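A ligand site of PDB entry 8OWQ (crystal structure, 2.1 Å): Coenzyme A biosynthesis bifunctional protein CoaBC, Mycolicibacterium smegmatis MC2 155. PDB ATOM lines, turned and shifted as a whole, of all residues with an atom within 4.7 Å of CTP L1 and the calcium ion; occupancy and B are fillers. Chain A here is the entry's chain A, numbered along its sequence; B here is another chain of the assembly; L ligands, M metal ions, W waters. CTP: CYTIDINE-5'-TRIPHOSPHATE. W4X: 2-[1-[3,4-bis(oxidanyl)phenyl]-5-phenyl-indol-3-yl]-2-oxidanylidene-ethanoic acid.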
ATOM      1  N   MET A  98       6.046 -16.437  27.349  1.00  0.00           N
ATOM      2  CA  MET A  98       7.483 -16.625  27.196  1.00  0.00           C
ATOM      3  C   MET A  98       8.093 -15.307  26.741  1.00  0.00           C
ATOM      4  O   MET A  98       8.272 -15.062  25.555  1.00  0.00           O
ATOM      5  CB  MET A  98       7.798 -17.738  26.208  1.00  0.00           C
ATOM      6  CG  MET A  98       7.612 -19.132  26.779  1.00  0.00           C
ATOM      7  SD  MET A  98       8.751 -19.602  28.094  1.00  0.00           S
ATOM      8  CE  MET A  98      10.268 -19.670  27.180  1.00  0.00           C
ATOM      9  N   ALA A  99       8.403 -14.440  27.689  1.00  0.00           N
ATOM     10  CA  ALA A  99       9.004 -13.179  27.314  1.00  0.00           C
ATOM     11  C   ALA A  99      10.525 -13.203  27.393  1.00  0.00           C
ATOM     12  O   ALA A  99      11.162 -12.293  26.847  1.00  0.00           O
ATOM     13  CB  ALA A  99       8.456 -12.039  28.168  1.00  0.00           C
ATOM     14  N   ALA A 100      11.122 -14.219  28.010  1.00  0.00           N
ATOM     15  CA  ALA A 100      12.570 -14.251  28.209  1.00  0.00           C
ATOM     16  C   ALA A 100      13.301 -14.355  26.870  1.00  0.00           C
ATOM     17  O   ALA A 100      12.792 -14.924  25.905  1.00  0.00           O
ATOM     18  CB  ALA A 100      12.950 -15.439  29.094  1.00  0.00           C
ATOM     19  N   VAL A 102      15.917 -16.492  25.592  1.00  0.00           N
ATOM     20  CA  VAL A 102      16.522 -17.768  25.976  1.00  0.00           C
ATOM     21  C   VAL A 102      17.668 -18.049  25.029  1.00  0.00           C
ATOM     22  O   VAL A 102      17.475 -18.126  23.804  1.00  0.00           O
ATOM     23  CB  VAL A 102      15.483 -18.904  25.949  1.00  0.00           C
ATOM     24  CG1 VAL A 102      16.065 -20.161  26.555  1.00  0.00           C
ATOM     25  CG2 VAL A 102      14.230 -18.514  26.706  1.00  0.00           C
ATOM     26  N   ALA A 103      18.874 -18.158  25.574  1.00  0.00           N
ATOM     27  CA  ALA A 103      20.045 -18.395  24.739  1.00  0.00           C
ATOM     28  C   ALA A 103      19.874 -19.650  23.908  1.00  0.00           C
ATOM     29  O   ALA A 103      19.584 -20.727  24.439  1.00  0.00           O
ATOM     30  CB  ALA A 103      21.294 -18.497  25.603  1.00  0.00           C
ATOM     31  N   ASP A 104      20.065 -19.523  22.606  1.00  0.00           N
ATOM     32  CA  ASP A 104      19.969 -20.700  21.770  1.00  0.00           C
ATOM     33  C   ASP A 104      21.235 -21.526  21.776  1.00  0.00           C
ATOM     34  O   ASP A 104      21.223 -22.622  21.211  1.00  0.00           O
ATOM     35  CB  ASP A 104      19.621 -20.324  20.324  1.00  0.00           C
ATOM     36  CG  ASP A 104      18.141 -20.086  20.135  1.00  0.00           C
ATOM     37  OD1 ASP A 104      17.347 -20.987  20.481  1.00  0.00           O
ATOM     38  OD2 ASP A 104      17.766 -18.990  19.656  1.00  0.00           O
ATOM     39  N   ASN A 130      20.811 -25.134  22.919  1.00  0.00           N
ATOM     40  CA  ASN A 130      19.861 -25.247  24.012  1.00  0.00           C
ATOM     41  C   ASN A 130      18.482 -25.541  23.456  1.00  0.00           C
ATOM     42  O   ASN A 130      18.169 -25.178  22.315  1.00  0.00           O
ATOM     43  CB  ASN A 130      19.826 -23.969  24.837  1.00  0.00           C
ATOM     44  CG  ASN A 130      21.117 -23.711  25.563  1.00  0.00           C
ATOM     45  OD1 ASN A 130      21.739 -24.633  26.104  1.00  0.00           O
ATOM     46  ND2 ASN A 130      21.542 -22.471  25.589  1.00  0.00           N
ATOM     47  N   ASP A 131      17.646 -26.180  24.266  1.00  0.00           N
ATOM     48  CA  ASP A 131      16.311 -26.548  23.838  1.00  0.00           C
ATOM     49  C   ASP A 131      15.439 -25.312  23.593  1.00  0.00           C
ATOM     50  O   ASP A 131      15.594 -24.274  24.241  1.00  0.00           O
ATOM     51  CB  ASP A 131      15.643 -27.442  24.870  1.00  0.00           C
ATOM     52  CG  ASP A 131      16.312 -28.782  24.996  1.00  0.00           C
ATOM     53  OD1 ASP A 131      17.243 -29.074  24.219  1.00  0.00           O
ATOM     54  OD2 ASP A 131      15.900 -29.580  25.865  1.00  0.00           O
ATOM     55  N   ASP A 132      14.526 -25.443  22.644  1.00  0.00           N
ATOM     56  CA  ASP A 132      13.483 -24.451  22.398  1.00  0.00           C
ATOM     57  C   ASP A 132      12.362 -24.717  23.389  1.00  0.00           C
ATOM     58  O   ASP A 132      11.586 -25.660  23.225  1.00  0.00           O
ATOM     59  CB  ASP A 132      13.006 -24.540  20.955  1.00  0.00           C
ATOM     60  CG  ASP A 132      12.102 -23.411  20.552  1.00  0.00           C
ATOM     61  OD1 ASP A 132      12.090 -23.088  19.355  1.00  0.00           O
ATOM     62  OD2 ASP A 132      11.380 -22.871  21.397  1.00  0.00           O
ATOM     63  N   VAL A 133      12.268 -23.870  24.428  1.00  0.00           N
ATOM     64  CA  VAL A 133      11.346 -24.100  25.541  1.00  0.00           C
ATOM     65  C   VAL A 133       9.900 -23.777  25.128  1.00  0.00           C
ATOM     66  O   VAL A 133       8.970 -24.510  25.457  1.00  0.00           O
ATOM     67  CB  VAL A 133      11.795 -23.274  26.752  1.00  0.00           C
ATOM     68  CG1 VAL A 133      10.881 -23.511  27.931  1.00  0.00           C
ATOM     69  CG2 VAL A 133      13.231 -23.576  27.102  1.00  0.00           C
ATOM     70  N   LEU A 134       9.697 -22.657  24.425  1.00  0.00           N
ATOM     71  CA  LEU A 134       8.383 -22.338  23.855  1.00  0.00           C
ATOM     72  C   LEU A 134       7.848 -23.468  22.990  1.00  0.00           C
ATOM     73  O   LEU A 134       6.671 -23.829  23.076  1.00  0.00           O
ATOM     74  CB  LEU A 134       8.440 -21.046  23.038  1.00  0.00           C
ATOM     75  CG  LEU A 134       7.136 -20.515  22.412  1.00  0.00           C
ATOM     76  CD1 LEU A 134       5.990 -20.428  23.407  1.00  0.00           C
ATOM     77  CD2 LEU A 134       7.366 -19.172  21.739  1.00  0.00           C
ATOM     78  N   GLY A 154       4.163 -16.286  22.866  1.00  0.00           N
ATOM     79  CA  GLY A 154       5.561 -16.029  22.634  1.00  0.00           C
ATOM     80  C   GLY A 154       5.866 -14.573  22.378  1.00  0.00           C
ATOM     81  O   GLY A 154       4.960 -13.793  22.057  1.00  0.00           O
ATOM     82  N   PHE A 155       7.135 -14.203  22.500  1.00  0.00           N
ATOM     83  CA  PHE A 155       7.602 -12.846  22.297  1.00  0.00           C
ATOM     84  C   PHE A 155       8.656 -12.842  21.200  1.00  0.00           C
ATOM     85  O   PHE A 155       9.328 -13.855  20.982  1.00  0.00           O
ATOM     86  CB  PHE A 155       8.213 -12.265  23.591  1.00  0.00           C
ATOM     87  CG  PHE A 155       7.250 -11.499  24.453  1.00  0.00           C
ATOM     88  CD1 PHE A 155       7.506 -10.180  24.797  1.00  0.00           C
ATOM     89  CD2 PHE A 155       6.102 -12.103  24.949  1.00  0.00           C
ATOM     90  CE1 PHE A 155       6.629  -9.465  25.616  1.00  0.00           C
ATOM     91  CE2 PHE A 155       5.217 -11.395  25.757  1.00  0.00           C
ATOM     92  CZ  PHE A 155       5.485 -10.080  26.095  1.00  0.00           C
ATOM     93  N   ALA A 156       8.806 -11.714  20.519  1.00  0.00           N
ATOM     94  CA  ALA A 156       9.836 -11.606  19.496  1.00  0.00           C
ATOM     95  C   ALA A 156      10.221 -10.143  19.351  1.00  0.00           C
ATOM     96  O   ALA A 156       9.392  -9.241  19.539  1.00  0.00           O
ATOM     97  CB  ALA A 156       9.376 -12.171  18.157  1.00  0.00           C
ATOM     98  N   GLU A 158      11.820  -8.056  16.327  1.00  0.00           N
ATOM     99  CA  GLU A 158      12.129  -8.178  14.907  1.00  0.00           C
ATOM    100  C   GLU A 158      12.495  -6.830  14.324  1.00  0.00           C
ATOM    101  O   GLU A 158      11.884  -5.811  14.650  1.00  0.00           O
ATOM    102  CB  GLU A 158      10.944  -8.758  14.118  1.00  0.00           C
ATOM    103  CG  GLU A 158      10.552 -10.191  14.447  1.00  0.00           C
ATOM    104  CD  GLU A 158      11.673 -11.199  14.229  1.00  0.00           C
ATOM    105  OE1 GLU A 158      11.690 -12.216  14.943  1.00  0.00           O
ATOM    106  OE2 GLU A 158      12.523 -10.980  13.345  1.00  0.00           O
ATOM    107  N   LYS A 173       7.874 -16.639  12.147  1.00  0.00           N
ATOM    108  CA  LYS A 173       8.139 -17.122  13.493  1.00  0.00           C
ATOM    109  C   LYS A 173       6.865 -17.633  14.176  1.00  0.00           C
ATOM    110  O   LYS A 173       6.880 -18.645  14.898  1.00  0.00           O
ATOM    111  CB  LYS A 173       8.786 -16.010  14.314  1.00  0.00           C
ATOM    112  CG  LYS A 173       9.438 -16.467  15.597  1.00  0.00           C
ATOM    113  CD  LYS A 173      10.374 -15.429  16.114  1.00  0.00           C
ATOM    114  CE  LYS A 173      11.693 -15.461  15.368  1.00  0.00           C
ATOM    115  NZ  LYS A 173      12.669 -14.483  15.920  1.00  0.00           N
ATOM    116  N   LYS A 177       6.775 -21.610  15.317  1.00  0.00           N
ATOM    117  CA  LYS A 177       6.730 -21.890  16.738  1.00  0.00           C
ATOM    118  C   LYS A 177       5.422 -22.578  17.149  1.00  0.00           C
ATOM    119  O   LYS A 177       5.436 -23.485  17.986  1.00  0.00           O
ATOM    120  CB  LYS A 177       6.930 -20.594  17.502  1.00  0.00           C
ATOM    121  CG  LYS A 177       8.327 -20.012  17.322  1.00  0.00           C
ATOM    122  CD  LYS A 177       9.278 -20.662  18.318  1.00  0.00           C
ATOM    123  CE  LYS A 177      10.615 -19.949  18.390  1.00  0.00           C
ATOM    124  NZ  LYS A 177      11.329 -20.363  19.650  1.00  0.00           N
ATOM    125  N   ARG B  30      24.201  -9.543  21.942  1.00  0.00           N
ATOM    126  CA  ARG B  30      24.852 -10.497  22.834  1.00  0.00           C
ATOM    127  C   ARG B  30      26.321 -10.169  23.008  1.00  0.00           C
ATOM    128  O   ARG B  30      26.881  -9.321  22.301  1.00  0.00           O
ATOM    129  CB  ARG B  30      24.647 -11.918  22.326  1.00  0.00           C
ATOM    130  CG  ARG B  30      23.180 -12.275  22.218  1.00  0.00           C
ATOM    131  CD  ARG B  30      22.895 -12.767  20.830  1.00  0.00           C
ATOM    132  NE  ARG B  30      21.505 -13.123  20.633  1.00  0.00           N
ATOM    133  CZ  ARG B  30      21.021 -13.594  19.483  1.00  0.00           C
ATOM    134  NH1 ARG B  30      19.734 -13.903  19.366  1.00  0.00           N
ATOM    135  NH2 ARG B  30      21.843 -13.739  18.444  1.00  0.00           N
ATOM    136  N   LYS B 114      21.790  -9.204  14.452  1.00  0.00           N
ATOM    137  CA  LYS B 114      21.548 -10.328  15.348  1.00  0.00           C
ATOM    138  C   LYS B 114      21.879 -11.638  14.652  1.00  0.00           C
ATOM    139  O   LYS B 114      21.309 -11.963  13.607  1.00  0.00           O
ATOM    140  CB  LYS B 114      20.082 -10.309  15.801  1.00  0.00           C
ATOM    141  CG  LYS B 114      19.782 -11.133  17.013  1.00  0.00           C
ATOM    142  CD  LYS B 114      18.506 -10.646  17.622  1.00  0.00           C
ATOM    143  CE  LYS B 114      17.482 -11.729  17.758  1.00  0.00           C
ATOM    144  NZ  LYS B 114      16.235 -11.158  18.334  1.00  0.00           N
ATOM    145  N   LYS B 116      21.933 -15.392  13.651  1.00  0.00           N
ATOM    146  CA  LYS B 116      20.958 -16.481  13.587  1.00  0.00           C
ATOM    147  C   LYS B 116      21.600 -17.594  12.763  1.00  0.00           C
ATOM    148  O   LYS B 116      21.628 -17.505  11.528  1.00  0.00           O
ATOM    149  CB  LYS B 116      19.641 -15.998  13.000  1.00  0.00           C
ATOM    150  CG  LYS B 116      18.663 -17.098  12.630  1.00  0.00           C
ATOM    151  CD  LYS B 116      17.268 -16.519  12.408  1.00  0.00           C
ATOM    152  CE  LYS B 116      17.292 -15.328  11.442  1.00  0.00           C
ATOM    153  NZ  LYS B 116      15.993 -15.108  10.732  1.00  0.00           N
HETATM  154  N1  CTP L   1      12.527 -19.229  23.245  1.00  0.00           N
HETATM  155  C2  CTP L   1      12.500 -20.439  23.911  1.00  0.00           C
HETATM  156  N3  CTP L   1      13.632 -21.237  23.902  1.00  0.00           N
HETATM  157  C4  CTP L   1      14.699 -20.941  23.073  1.00  0.00           C
HETATM  158  C5  CTP L   1      14.655 -19.799  22.275  1.00  0.00           C
HETATM  159  C6  CTP L   1      13.516 -18.994  22.314  1.00  0.00           C
HETATM  160  O2  CTP L   1      11.464 -20.783  24.490  1.00  0.00           O
HETATM  161  N4  CTP L   1      15.764 -21.729  23.041  1.00  0.00           N
HETATM  162  C1' CTP L   1      11.283 -18.450  23.201  1.00  0.00           C
HETATM  163  C2' CTP L   1      11.477 -17.009  23.647  1.00  0.00           C
HETATM  164  O2' CTP L   1      11.237 -16.780  25.030  1.00  0.00           O
HETATM  165  C3' CTP L   1      10.514 -16.241  22.768  1.00  0.00           C
HETATM  166  C4' CTP L   1      10.329 -17.123  21.548  1.00  0.00           C
HETATM  167  O4' CTP L   1      10.856 -18.400  21.853  1.00  0.00           O
HETATM  168  O3' CTP L   1       9.250 -16.099  23.387  1.00  0.00           O
HETATM  169  C5' CTP L   1      10.990 -16.575  20.296  1.00  0.00           C
HETATM  170  O5' CTP L   1      12.290 -16.058  20.563  1.00  0.00           O
HETATM  171  PA  CTP L   1      13.287 -15.877  19.295  1.00  0.00           P
HETATM  172  O1A CTP L   1      14.727 -15.792  19.743  1.00  0.00           O
HETATM  173  O2A CTP L   1      12.888 -14.743  18.378  1.00  0.00           O
HETATM  174  O3A CTP L   1      13.048 -17.276  18.572  1.00  0.00           O
HETATM  175  PB  CTP L   1      14.167 -17.829  17.582  1.00  0.00           P
HETATM  176  O1B CTP L   1      15.066 -18.780  18.354  1.00  0.00           O
HETATM  177  O2B CTP L   1      13.443 -18.568  16.489  1.00  0.00           O
HETATM  178  O3B CTP L   1      14.906 -16.431  17.109  1.00  0.00           O
HETATM  179  PG  CTP L   1      15.766 -16.061  15.763  1.00  0.00           P
HETATM  180  O1G CTP L   1      16.751 -17.183  15.509  1.00  0.00           O
HETATM  181  O2G CTP L   1      14.867 -15.855  14.561  1.00  0.00           O
HETATM  182  O3G CTP L   1      16.532 -14.769  15.961  1.00  0.00           O
HETATM  183  C10 W4X L   2      24.287 -16.549  20.070  1.00  0.00           C
HETATM  184  C13 W4X L   2      22.574 -17.305  18.862  1.00  0.00           C
HETATM  185  C17 W4X L   2      26.910 -15.790  18.333  1.00  0.00           C
HETATM  186  C20 W4X L   2      27.900 -18.132  17.271  1.00  0.00           C
HETATM  187  C21 W4X L   2      26.625 -18.117  17.798  1.00  0.00           C
HETATM  188  C24 W4X L   2      21.187 -17.695  18.339  1.00  0.00           C
HETATM  189  C01 W4X L   2      20.153 -14.576  24.623  1.00  0.00           C
HETATM  190  C02 W4X L   2      20.770 -14.667  25.852  1.00  0.00           C
HETATM  191  C03 W4X L   2      22.073 -15.147  25.966  1.00  0.00           C
HETATM  192  C04 W4X L   2      22.754 -15.546  24.833  1.00  0.00           C
HETATM  193  C05 W4X L   2      22.127 -15.473  23.612  1.00  0.00           C
HETATM  194  C06 W4X L   2      20.834 -14.984  23.495  1.00  0.00           C
HETATM  195  C07 W4X L   2      22.871 -15.873  22.363  1.00  0.00           C
HETATM  196  C08 W4X L   2      24.238 -15.664  22.321  1.00  0.00           C
HETATM  197  C09 W4X L   2      24.955 -16.007  21.186  1.00  0.00           C
HETATM  198  C11 W4X L   2      22.918 -16.744  20.115  1.00  0.00           C
HETATM  199  C12 W4X L   2      22.189 -16.398  21.257  1.00  0.00           C
HETATM  200  C14 W4X L   2      23.750 -17.400  18.144  1.00  0.00           C
HETATM  201  C16 W4X L   2      26.121 -16.952  18.348  1.00  0.00           C
HETATM  202  C18 W4X L   2      28.199 -15.823  17.797  1.00  0.00           C
HETATM  203  C19 W4X L   2      28.700 -17.000  17.265  1.00  0.00           C
HETATM  204  C25 W4X L   2      21.063 -18.312  16.924  1.00  0.00           C
HETATM  205  N15 W4X L   2      24.757 -16.962  18.869  1.00  0.00           N
HETATM  206  O22 W4X L   2      28.423 -19.312  16.735  1.00  0.00           O
HETATM  207  O23 W4X L   2      29.988 -17.089  16.714  1.00  0.00           O
HETATM  208  O26 W4X L   2      19.947 -18.296  16.325  1.00  0.00           O
HETATM  209  O27 W4X L   2      22.052 -18.837  16.340  1.00  0.00           O
HETATM  210  O28 W4X L   2      20.234 -17.483  19.005  1.00  0.00           O
HETATM  211  C10 W4X L   3      11.773  -9.241  23.957  1.00  0.00           C
HETATM  212  C13 W4X L   3      12.564  -8.628  25.959  1.00  0.00           C
HETATM  213  C17 W4X L   3      12.964 -12.348  23.259  1.00  0.00           C
HETATM  214  C20 W4X L   3      15.215 -11.478  21.866  1.00  0.00           C
HETATM  215  C21 W4X L   3      14.534 -10.633  22.713  1.00  0.00           C
HETATM  216  C24 W4X L   3      12.791  -7.944  27.335  1.00  0.00           C
HETATM  217  C01 W4X L   3       7.642  -4.238  23.803  1.00  0.00           C
HETATM  218  C02 W4X L   3       6.441  -4.667  23.241  1.00  0.00           C
HETATM  219  C03 W4X L   3       6.285  -5.982  22.848  1.00  0.00           C
HETATM  220  C04 W4X L   3       7.318  -6.877  23.042  1.00  0.00           C
HETATM  221  C05 W4X L   3       8.508  -6.461  23.621  1.00  0.00           C
HETATM  222  C06 W4X L   3       8.687  -5.128  23.986  1.00  0.00           C
HETATM  223  C07 W4X L   3       9.655  -7.444  23.790  1.00  0.00           C
HETATM  224  C08 W4X L   3       9.896  -8.321  22.746  1.00  0.00           C
HETATM  225  C09 W4X L   3      10.950  -9.224  22.830  1.00  0.00           C
HETATM  226  C11 W4X L   3      11.554  -8.359  24.992  1.00  0.00           C
HETATM  227  C12 W4X L   3      10.488  -7.443  24.908  1.00  0.00           C
HETATM  228  C14 W4X L   3      13.307  -9.669  25.428  1.00  0.00           C
HETATM  229  C16 W4X L   3      13.422 -11.044  23.410  1.00  0.00           C
HETATM  230  C18 W4X L   3      13.647 -13.215  22.414  1.00  0.00           C
HETATM  231  C19 W4X L   3      14.766 -12.767  21.720  1.00  0.00           C
HETATM  232  C25 W4X L   3      11.632  -7.289  28.049  1.00  0.00           C
HETATM  233  N15 W4X L   3      12.826 -10.025  24.256  1.00  0.00           N
HETATM  234  O22 W4X L   3      16.346 -11.035  21.165  1.00  0.00           O
HETATM  235  O23 W4X L   3      15.469 -13.616  20.868  1.00  0.00           O
HETATM  236  O26 W4X L   3      11.435  -6.056  27.913  1.00  0.00           O
HETATM  237  O27 W4X L   3      10.903  -8.018  28.773  1.00  0.00           O
HETATM  238  O28 W4X L   3      13.839  -7.907  27.884  1.00  0.00           O
HETATM  239 CA    CA M   1      18.032 -17.677  17.822  1.00  0.00          CA
HETATM  240  O   HOH W   1      13.772 -13.252  12.556  1.00  0.00           O
HETATM  241  O   HOH W   2      16.941 -16.002  19.113  1.00  0.00           O
HETATM  242  O   HOH W   3      15.121 -16.308  22.822  1.00  0.00           O
HETATM  243  O   HOH W   4      17.396 -13.025  13.987  1.00  0.00           O
HETATM  244  O   HOH W   5      18.925 -15.207  16.404  1.00  0.00           O
HETATM  245  O   HOH W   6      13.278 -12.120  18.577  1.00  0.00           O
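The side-chain amino group (NZ) of Lys 173 lies within salt-bridge range of an oxygen (O2A) of CTP L1 (2.5 Å).
The backbone carbonyl oxygen (O) of Ala 100 sits at hydrogen-bond distance from an oxygen (O2') of CTP L1.
N of Leu 134 lies within hydrogen-bond range of O2 of CTP L1, at 2.6 Å.
The backbone carbonyl oxygen (O) of Met 98 lies within hydrogen-bond range of an oxygen (O3') of CTP L1, 2.6 Å away.
The backbone carbonyl oxygen of Asp 131 is in hydrogen-bond range of a nitrogen (N4) of CTP L1, at 2.8 Å.
An oxygen (O3') of CTP L1 is in hydrogen-bond range of the backbone NH (N) of Phe 155.
O3' of CTP L1 lies close to O of Phe 155 (3.3 Å).
O4' of CTP L1 is in hydrogen-bond range of NZ of Lys 177 (3.0 Å).
A nitrogen (N3) of CTP L1 is in hydrogen-bond range of the backbone NH of Val 133 (3.0 Å).
O22 of W4X L3 is in hydrogen-bond range of NZ of Lys 114 of chain B (2.8 Å).
Residues that only touch CTP L1: Lys 116 of chain B, Asp 132, Val 102, Lys 114 of chain B and Gly 154.
Within 4 Å of CTP L1: Met 98, Ala 100, Val 102, Asp 104, Asp 131, Asp 132, Val 133, Leu 134, Gly 154, Phe 155, Lys 173, Lys 177, Lys 114 of chain B and Lys 116 of chain B.
O of Asp 104 sits at hydrogen-bond distance from N of Asn 130, at 3.1 Å.
The side-chain carboxylate (OE1) of Glu 158 is in salt-bridge range of the side-chain amino group (NZ) of Lys 173 (2.7 Å).
N of Leu 134 lies within hydrogen-bond range of OD2 of Asp 132, 3.5 Å away.
N of Phe 155 is in hydrogen-bond range of O of Met 98 (3.4 Å).
The side-chain amino group (NZ) of Lys 177 is in salt-bridge range of the side-chain carboxylate (OD1) of Asp 132, 2.8 Å away.
An oxygen (O23) of W4X L3 sits at hydrogen-bond distance from an oxygen (O1A) of CTP L1 (2.6 Å).
OD2 of Asp 104 binds the calcium ion (2.3 Å).
Water W2 is bound to the calcium ion (2.4 Å).
The calcium ion is bound by O28 of W4X L2 (2.5 Å).
O26 of W4X L2 is bound to the calcium ion.
O1G of CTP L1 is bound to the calcium ion (2.7 Å).
Slightly farther from the calcium ion lies water W5 (3.0 Å).
Water W2 lies within hydrogen-bond range of an oxygen (O3B) of CTP L1 and an oxygen (O23) of W4X L3.
Water W5 lies within hydrogen-bond range of O3G of CTP L1 (2.5 Å) and NH1 of Arg 30 of chain B (3.3 Å).
Water W6 bridges O2A of CTP L1 and NZ of Lys 114 of chain B.
Water W3 lies within hydrogen-bond range of N of Val 102 (2.9 Å), O1A of CTP L1 (3.1 Å) and O23 of W4X L3 (3.3 Å).
Water W1 lies within hydrogen-bond range of the side-chain carboxylate of Glu 158 (2.7 Å), the side-chain amino group of Lys 116 of chain B (3.4 Å) and an oxygen (O2G) of CTP L1 (3.5 Å).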
